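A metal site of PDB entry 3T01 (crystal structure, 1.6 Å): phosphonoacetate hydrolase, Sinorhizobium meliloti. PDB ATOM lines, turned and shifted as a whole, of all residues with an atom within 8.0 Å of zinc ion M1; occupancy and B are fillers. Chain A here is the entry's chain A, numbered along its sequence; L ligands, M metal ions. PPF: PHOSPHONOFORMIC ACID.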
ATOM      1  N   CYS A  30     -22.901  16.376 -10.378  1.00  0.00           N
ATOM      2  CA  CYS A  30     -23.314  17.527 -11.156  1.00  0.00           C
ATOM      3  C   CYS A  30     -24.833  17.563 -11.212  1.00  0.00           C
ATOM      4  O   CYS A  30     -25.455  16.758 -11.915  1.00  0.00           O
ATOM      5  CB  CYS A  30     -22.728  17.460 -12.571  1.00  0.00           C
ATOM      6  SG  CYS A  30     -23.252  18.821 -13.630  1.00  0.00           S
ATOM      7  N   LEU A  31     -25.404  18.484 -10.454  1.00  0.00           N
ATOM      8  CA  LEU A  31     -26.837  18.766 -10.501  1.00  0.00           C
ATOM      9  C   LEU A  31     -27.091  19.723 -11.654  1.00  0.00           C
ATOM     10  O   LEU A  31     -26.923  20.946 -11.523  1.00  0.00           O
ATOM     11  CB  LEU A  31     -27.326  19.335  -9.151  1.00  0.00           C
ATOM     12  CG  LEU A  31     -27.167  18.444  -7.913  1.00  0.00           C
ATOM     13  CD1 LEU A  31     -27.626  19.187  -6.663  1.00  0.00           C
ATOM     14  CD2 LEU A  31     -27.924  17.122  -8.067  1.00  0.00           C
ATOM     15  N   ASP A  32     -27.449  19.158 -12.794  1.00  0.00           N
ATOM     16  CA  ASP A  32     -27.649  19.916 -14.026  1.00  0.00           C
ATOM     17  C   ASP A  32     -28.649  21.051 -13.804  1.00  0.00           C
ATOM     18  O   ASP A  32     -29.765  20.838 -13.335  1.00  0.00           O
ATOM     19  CB  ASP A  32     -28.119  18.969 -15.126  1.00  0.00           C
ATOM     20  CG  ASP A  32     -27.855  19.498 -16.516  1.00  0.00           C
ATOM     21  OD1 ASP A  32     -28.058  20.705 -16.753  1.00  0.00           O
ATOM     22  OD2 ASP A  32     -27.445  18.685 -17.372  1.00  0.00           O
ATOM     23  N   GLY A  33     -28.225  22.275 -14.137  1.00  0.00           N
ATOM     24  CA  GLY A  33     -29.084  23.444 -14.035  1.00  0.00           C
ATOM     25  C   GLY A  33     -29.466  23.877 -12.627  1.00  0.00           C
ATOM     26  O   GLY A  33     -30.432  24.631 -12.456  1.00  0.00           O
ATOM     27  N   CYS A  34     -28.711  23.437 -11.627  1.00  0.00           N
ATOM     28  CA  CYS A  34     -29.034  23.776 -10.247  1.00  0.00           C
ATOM     29  C   CYS A  34     -28.622  25.188  -9.863  1.00  0.00           C
ATOM     30  O   CYS A  34     -27.595  25.400  -9.224  1.00  0.00           O
ATOM     31  CB  CYS A  34     -28.435  22.754  -9.275  1.00  0.00           C
ATOM     32  SG  CYS A  34     -29.091  22.930  -7.599  1.00  0.00           S
ATOM     33  N   SER A  69     -22.410  28.998 -20.361  1.00  0.00           N
ATOM     34  CA  SER A  69     -22.954  28.196 -19.254  1.00  0.00           C
ATOM     35  C   SER A  69     -23.952  27.173 -19.778  1.00  0.00           C
ATOM     36  O   SER A  69     -25.145  27.198 -19.443  1.00  0.00           O
ATOM     37  CB  SER A  69     -23.513  29.100 -18.148  1.00  0.00           C
ATOM     38  OG  SER A  69     -24.504  29.997 -18.640  1.00  0.00           O
ATOM     39  N   PHE A  70     -23.438  26.265 -20.606  1.00  0.00           N
ATOM     40  CA  PHE A  70     -24.207  25.176 -21.208  1.00  0.00           C
ATOM     41  C   PHE A  70     -23.711  23.817 -20.686  1.00  0.00           C
ATOM     42  O   PHE A  70     -22.633  23.728 -20.094  1.00  0.00           O
ATOM     43  CB  PHE A  70     -24.115  25.196 -22.735  1.00  0.00           C
ATOM     44  CG  PHE A  70     -24.811  26.380 -23.390  1.00  0.00           C
ATOM     45  CD1 PHE A  70     -26.067  26.808 -22.969  1.00  0.00           C
ATOM     46  CD2 PHE A  70     -24.204  27.027 -24.458  1.00  0.00           C
ATOM     47  CE1 PHE A  70     -26.695  27.898 -23.588  1.00  0.00           C
ATOM     48  CE2 PHE A  70     -24.819  28.113 -25.092  1.00  0.00           C
ATOM     49  CZ  PHE A  70     -26.064  28.549 -24.650  1.00  0.00           C
ATOM     50  N   THR A  71     -24.504  22.785 -20.928  1.00  0.00           N
ATOM     51  CA  THR A  71     -24.278  21.462 -20.355  1.00  0.00           C
ATOM     52  C   THR A  71     -23.005  20.764 -20.810  1.00  0.00           C
ATOM     53  O   THR A  71     -22.209  20.325 -19.967  1.00  0.00           O
ATOM     54  CB  THR A  71     -25.493  20.552 -20.599  1.00  0.00           C
ATOM     55  OG1 THR A  71     -26.627  21.132 -19.940  1.00  0.00           O
ATOM     56  CG2 THR A  71     -25.254  19.129 -20.065  1.00  0.00           C
ATOM     57  N   ASN A  72     -22.819  20.640 -22.122  1.00  0.00           N
ATOM     58  CA  ASN A  72     -21.667  19.894 -22.627  1.00  0.00           C
ATOM     59  C   ASN A  72     -20.317  20.515 -22.263  1.00  0.00           C
ATOM     60  O   ASN A  72     -19.462  19.821 -21.725  1.00  0.00           O
ATOM     61  CB  ASN A  72     -21.764  19.618 -24.128  1.00  0.00           C
ATOM     62  CG  ASN A  72     -22.868  18.646 -24.487  1.00  0.00           C
ATOM     63  OD1 ASN A  72     -23.938  18.637 -23.865  1.00  0.00           O
ATOM     64  ND2 ASN A  72     -22.631  17.817 -25.506  1.00  0.00           N
ATOM     65  N   PRO A  73     -20.137  21.831 -22.526  1.00  0.00           N
ATOM     66  CA  PRO A  73     -18.835  22.424 -22.181  1.00  0.00           C
ATOM     67  C   PRO A  73     -18.532  22.320 -20.688  1.00  0.00           C
ATOM     68  O   PRO A  73     -17.383  22.072 -20.298  1.00  0.00           O
ATOM     69  CB  PRO A  73     -18.989  23.891 -22.585  1.00  0.00           C
ATOM     70  CG  PRO A  73     -20.110  23.923 -23.542  1.00  0.00           C
ATOM     71  CD  PRO A  73     -21.030  22.815 -23.166  1.00  0.00           C
ATOM     72  N   ASN A  74     -19.541  22.481 -19.847  1.00  0.00           N
ATOM     73  CA  ASN A  74     -19.309  22.417 -18.416  1.00  0.00           C
ATOM     74  C   ASN A  74     -19.097  21.002 -17.882  1.00  0.00           C
ATOM     75  O   ASN A  74     -18.206  20.795 -17.044  1.00  0.00           O
ATOM     76  CB  ASN A  74     -20.398  23.155 -17.673  1.00  0.00           C
ATOM     77  CG  ASN A  74     -20.171  24.647 -17.689  1.00  0.00           C
ATOM     78  OD1 ASN A  74     -20.719  25.376 -18.532  1.00  0.00           O
ATOM     79  ND2 ASN A  74     -19.329  25.098 -16.797  1.00  0.00           N
ATOM     80  N   ASN A  75     -19.860  20.042 -18.382  1.00  0.00           N
ATOM     81  CA  ASN A  75     -19.615  18.651 -17.992  1.00  0.00           C
ATOM     82  C   ASN A  75     -18.213  18.190 -18.368  1.00  0.00           C
ATOM     83  O   ASN A  75     -17.542  17.525 -17.575  1.00  0.00           O
ATOM     84  CB  ASN A  75     -20.649  17.709 -18.574  1.00  0.00           C
ATOM     85  CG  ASN A  75     -21.864  17.591 -17.687  1.00  0.00           C
ATOM     86  OD1 ASN A  75     -22.849  18.335 -17.833  1.00  0.00           O
ATOM     87  ND2 ASN A  75     -21.813  16.667 -16.755  1.00  0.00           N
ATOM     88  N   LEU A 136     -23.832  12.231 -23.674  1.00  0.00           N
ATOM     89  CA  LEU A 136     -22.696  12.659 -22.856  1.00  0.00           C
ATOM     90  C   LEU A 136     -21.831  11.464 -22.419  1.00  0.00           C
ATOM     91  O   LEU A 136     -20.660  11.616 -22.059  1.00  0.00           O
ATOM     92  CB  LEU A 136     -23.210  13.439 -21.641  1.00  0.00           C
ATOM     93  CG  LEU A 136     -22.313  14.172 -20.641  1.00  0.00           C
ATOM     94  CD1 LEU A 136     -21.319  15.095 -21.317  1.00  0.00           C
ATOM     95  CD2 LEU A 136     -23.184  14.948 -19.660  1.00  0.00           C
ATOM     96  N   THR A 211     -23.952  12.654 -13.105  1.00  0.00           N
ATOM     97  CA  THR A 211     -24.456  13.861 -13.762  1.00  0.00           C
ATOM     98  C   THR A 211     -25.865  13.650 -14.288  1.00  0.00           C
ATOM     99  O   THR A 211     -26.187  12.581 -14.801  1.00  0.00           O
ATOM    100  CB  THR A 211     -23.468  14.398 -14.841  1.00  0.00           C
ATOM    101  OG1 THR A 211     -23.933  15.665 -15.317  1.00  0.00           O
ATOM    102  CG2 THR A 211     -23.326  13.423 -16.006  1.00  0.00           C
ATOM    103  N   THR A 212     -26.693  14.675 -14.125  1.00  0.00           N
ATOM    104  CA  THR A 212     -28.139  14.554 -14.326  1.00  0.00           C
ATOM    105  C   THR A 212     -28.558  15.327 -15.579  1.00  0.00           C
ATOM    106  O   THR A 212     -27.714  15.627 -16.416  1.00  0.00           O
ATOM    107  CB  THR A 212     -28.865  15.087 -13.079  1.00  0.00           C
ATOM    108  OG1 THR A 212     -28.500  16.453 -12.862  1.00  0.00           O
ATOM    109  CG2 THR A 212     -28.465  14.278 -11.846  1.00  0.00           C
ATOM    110  N   THR A 213     -29.855  15.602 -15.738  1.00  0.00           N
ATOM    111  CA  THR A 213     -30.302  16.551 -16.769  1.00  0.00           C
ATOM    112  C   THR A 213     -31.097  17.664 -16.123  1.00  0.00           C
ATOM    113  O   THR A 213     -31.547  17.528 -14.974  1.00  0.00           O
ATOM    114  CB  THR A 213     -31.181  15.932 -17.901  1.00  0.00           C
ATOM    115  OG1 THR A 213     -32.534  15.814 -17.455  1.00  0.00           O
ATOM    116  CG2 THR A 213     -30.653  14.589 -18.338  1.00  0.00           C
ATOM    117  N   ASP A 214     -31.266  18.762 -16.859  1.00  0.00           N
ATOM    118  CA  ASP A 214     -31.974  19.925 -16.331  1.00  0.00           C
ATOM    119  C   ASP A 214     -33.433  19.995 -16.787  1.00  0.00           C
ATOM    120  O   ASP A 214     -34.002  21.084 -16.856  1.00  0.00           O
ATOM    121  CB  ASP A 214     -31.214  21.224 -16.636  1.00  0.00           C
ATOM    122  CG  ASP A 214     -30.991  21.467 -18.120  1.00  0.00           C
ATOM    123  OD1 ASP A 214     -31.426  20.658 -18.972  1.00  0.00           O
ATOM    124  OD2 ASP A 214     -30.340  22.494 -18.447  1.00  0.00           O
ATOM    125  N   TYR A 215     -34.024  18.833 -17.081  1.00  0.00           N
ATOM    126  CA  TYR A 215     -35.436  18.766 -17.463  1.00  0.00           C
ATOM    127  C   TYR A 215     -36.346  19.511 -16.493  1.00  0.00           C
ATOM    128  O   TYR A 215     -37.118  20.386 -16.893  1.00  0.00           O
ATOM    129  CB  TYR A 215     -35.887  17.306 -17.602  1.00  0.00           C
ATOM    130  CG  TYR A 215     -37.392  17.184 -17.773  1.00  0.00           C
ATOM    131  CD1 TYR A 215     -37.986  17.425 -19.006  1.00  0.00           C
ATOM    132  CD2 TYR A 215     -38.202  16.832 -16.695  1.00  0.00           C
ATOM    133  CE1 TYR A 215     -39.361  17.315 -19.161  1.00  0.00           C
ATOM    134  CE2 TYR A 215     -39.583  16.725 -16.843  1.00  0.00           C
ATOM    135  CZ  TYR A 215     -40.147  16.967 -18.076  1.00  0.00           C
ATOM    136  OH  TYR A 215     -41.512  16.864 -18.239  1.00  0.00           O
ATOM    137  N   GLN A 217     -35.596  21.660 -14.161  1.00  0.00           N
ATOM    138  CA  GLN A 217     -35.184  23.033 -13.918  1.00  0.00           C
ATOM    139  C   GLN A 217     -35.588  23.985 -15.051  1.00  0.00           C
ATOM    140  O   GLN A 217     -35.871  25.157 -14.808  1.00  0.00           O
ATOM    141  CB  GLN A 217     -33.676  23.086 -13.624  1.00  0.00           C
ATOM    142  CG  GLN A 217     -33.265  22.329 -12.329  1.00  0.00           C
ATOM    143  CD  GLN A 217     -33.370  20.813 -12.444  1.00  0.00           C
ATOM    144  OE1 GLN A 217     -33.277  20.236 -13.524  1.00  0.00           O
ATOM    145  NE2 GLN A 217     -33.547  20.160 -11.308  1.00  0.00           N
ATOM    146  N   HIS A 218     -35.627  23.473 -16.283  1.00  0.00           N
ATOM    147  CA  HIS A 218     -36.161  24.268 -17.397  1.00  0.00           C
ATOM    148  C   HIS A 218     -37.658  24.518 -17.229  1.00  0.00           C
ATOM    149  O   HIS A 218     -38.164  25.536 -17.687  1.00  0.00           O
ATOM    150  CB  HIS A 218     -35.906  23.595 -18.741  1.00  0.00           C
ATOM    151  CG  HIS A 218     -34.557  23.874 -19.342  1.00  0.00           C
ATOM    152  ND1 HIS A 218     -34.226  25.062 -19.938  1.00  0.00           N
ATOM    153  CD2 HIS A 218     -33.461  23.082 -19.453  1.00  0.00           C
ATOM    154  CE1 HIS A 218     -32.984  25.016 -20.374  1.00  0.00           C
ATOM    155  NE2 HIS A 218     -32.496  23.815 -20.106  1.00  0.00           N
ATOM    156  N   ALA A 252     -22.789  22.148  -9.916  1.00  0.00           N
ATOM    157  CA  ALA A 252     -23.651  22.151 -11.086  1.00  0.00           C
ATOM    158  C   ALA A 252     -22.858  22.575 -12.302  1.00  0.00           C
ATOM    159  O   ALA A 252     -21.796  23.201 -12.182  1.00  0.00           O
ATOM    160  CB  ALA A 252     -24.844  23.095 -10.864  1.00  0.00           C
ATOM    161  N   ASP A 253     -23.374  22.217 -13.472  1.00  0.00           N
ATOM    162  CA  ASP A 253     -22.774  22.647 -14.722  1.00  0.00           C
ATOM    163  C   ASP A 253     -23.066  24.118 -15.058  1.00  0.00           C
ATOM    164  O   ASP A 253     -22.283  24.772 -15.722  1.00  0.00           O
ATOM    165  CB  ASP A 253     -23.140  21.706 -15.883  1.00  0.00           C
ATOM    166  CG  ASP A 253     -24.643  21.571 -16.103  1.00  0.00           C
ATOM    167  OD1 ASP A 253     -25.456  21.976 -15.238  1.00  0.00           O
ATOM    168  OD2 ASP A 253     -25.008  21.045 -17.167  1.00  0.00           O
ATOM    169  N   HIS A 254     -24.211  24.609 -14.572  1.00  0.00           N
ATOM    170  CA  HIS A 254     -24.682  25.974 -14.797  1.00  0.00           C
ATOM    171  C   HIS A 254     -25.958  26.165 -13.997  1.00  0.00           C
ATOM    172  O   HIS A 254     -26.554  25.181 -13.512  1.00  0.00           O
ATOM    173  CB  HIS A 254     -25.000  26.220 -16.281  1.00  0.00           C
ATOM    174  CG  HIS A 254     -25.947  25.220 -16.851  1.00  0.00           C
ATOM    175  ND1 HIS A 254     -27.306  25.271 -16.645  1.00  0.00           N
ATOM    176  CD2 HIS A 254     -25.717  24.112 -17.604  1.00  0.00           C
ATOM    177  CE1 HIS A 254     -27.877  24.245 -17.242  1.00  0.00           C
ATOM    178  NE2 HIS A 254     -26.942  23.522 -17.824  1.00  0.00           N
ATOM    179  N   GLY A 255     -26.381  27.418 -13.866  1.00  0.00           N
ATOM    180  CA  GLY A 255     -27.610  27.767 -13.173  1.00  0.00           C
ATOM    181  C   GLY A 255     -28.791  27.819 -14.121  1.00  0.00           C
ATOM    182  O   GLY A 255     -28.792  27.179 -15.166  1.00  0.00           O
ATOM    183  N   MET A 256     -29.816  28.581 -13.742  1.00  0.00           N
ATOM    184  CA  MET A 256     -31.050  28.638 -14.518  1.00  0.00           C
ATOM    185  C   MET A 256     -31.785  29.917 -14.135  1.00  0.00           C
ATOM    186  O   MET A 256     -31.902  30.245 -12.954  1.00  0.00           O
ATOM    187  CB  MET A 256     -31.930  27.407 -14.232  1.00  0.00           C
ATOM    188  CG  MET A 256     -33.143  27.239 -15.163  1.00  0.00           C
ATOM    189  SD  MET A 256     -32.716  26.664 -16.829  1.00  0.00           S
ATOM    190  CE  MET A 256     -32.128  25.004 -16.512  1.00  0.00           C
ATOM    191  N   HIS A 380     -30.418  29.136 -19.838  1.00  0.00           N
ATOM    192  CA  HIS A 380     -29.081  29.401 -19.340  1.00  0.00           C
ATOM    193  C   HIS A 380     -28.157  29.701 -20.520  1.00  0.00           C
ATOM    194  O   HIS A 380     -28.639  29.890 -21.649  1.00  0.00           O
ATOM    195  CB  HIS A 380     -28.586  28.204 -18.527  1.00  0.00           C
ATOM    196  CG  HIS A 380     -28.776  26.886 -19.199  1.00  0.00           C
ATOM    197  ND1 HIS A 380     -27.769  26.260 -19.901  1.00  0.00           N
ATOM    198  CD2 HIS A 380     -29.865  26.080 -19.310  1.00  0.00           C
ATOM    199  CE1 HIS A 380     -28.225  25.120 -20.399  1.00  0.00           C
ATOM    200  NE2 HIS A 380     -29.496  24.992 -20.055  1.00  0.00           N
HETATM  201  C1  PPF L   1     -27.684  22.072 -22.909  1.00  0.00           C
HETATM  202  O1  PPF L   1     -29.779  20.623 -23.318  1.00  0.00           O
HETATM  203  O2  PPF L   1     -29.986  22.654 -21.816  1.00  0.00           O
HETATM  204  O3  PPF L   1     -28.697  20.616 -21.051  1.00  0.00           O
HETATM  205  O4  PPF L   1     -27.218  21.496 -23.918  1.00  0.00           O
HETATM  206  O5  PPF L   1     -27.095  23.045 -22.403  1.00  0.00           O
HETATM  207  P1  PPF L   1     -29.145  21.454 -22.228  1.00  0.00           P
HETATM  208 ZN    ZN M   1     -26.819  21.511 -18.000  1.00  0.00          ZN
HETATM  209 ZN    ZN M   2     -30.546  23.236 -20.230  1.00  0.00          ZN
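Residues that only touch zinc ion M1: Asp 214 (3.7 Å). The nearest printed residue that does not touch zinc ion M1 is Gly 33 (4.2 Å).
An oxygen (O3) of the ligand lies close to the side-chain hydroxyl of Thr 71, at 2.4 Å. O5 of the ligand sits at hydrogen-bond distance from N of Thr 71, at 3.0 Å.
Zinc ion M1 is bound by the side-chain carboxylate (OD1) of Asp 32, the side-chain hydroxyl (OG1) of Thr 71, a ring nitrogen (NE2) of His 254 and the side-chain carboxylate (OD2) of Asp 253.
The backbone NH (N) of Gly 33 lies within hydrogen-bond range of the side-chain carboxylate (OD1) of Asp 253 (3.0 Å). The side-chain hydroxyl (OG1) of Thr 212 sits at hydrogen-bond distance from the backbone NH (N) of Asp 32 (2.9 Å). The backbone carbonyl oxygen (O) of Thr 71 lies close to the side-chain amide oxygen (OD1) of Asn 75 (3.0 Å). The backbone carbonyl oxygen (O) of His 254 sits close to the backbone NH (N) of Gly 33, at 3.4 Å. The side-chain sulfur (SG) of Cys 30 lies within hydrogen-bond range of the backbone NH (N) of Asp 253, 3.4 Å away. ND1 of His 380 sits close to ND1 of His 254. O of Asp 253 sits close to ND2 of Asn 74 (3.2 Å). The backbone carbonyl oxygen (O) of His 254 sits at hydrogen-bond distance from the backbone NH (N) of Cys 34 (3.4 Å).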
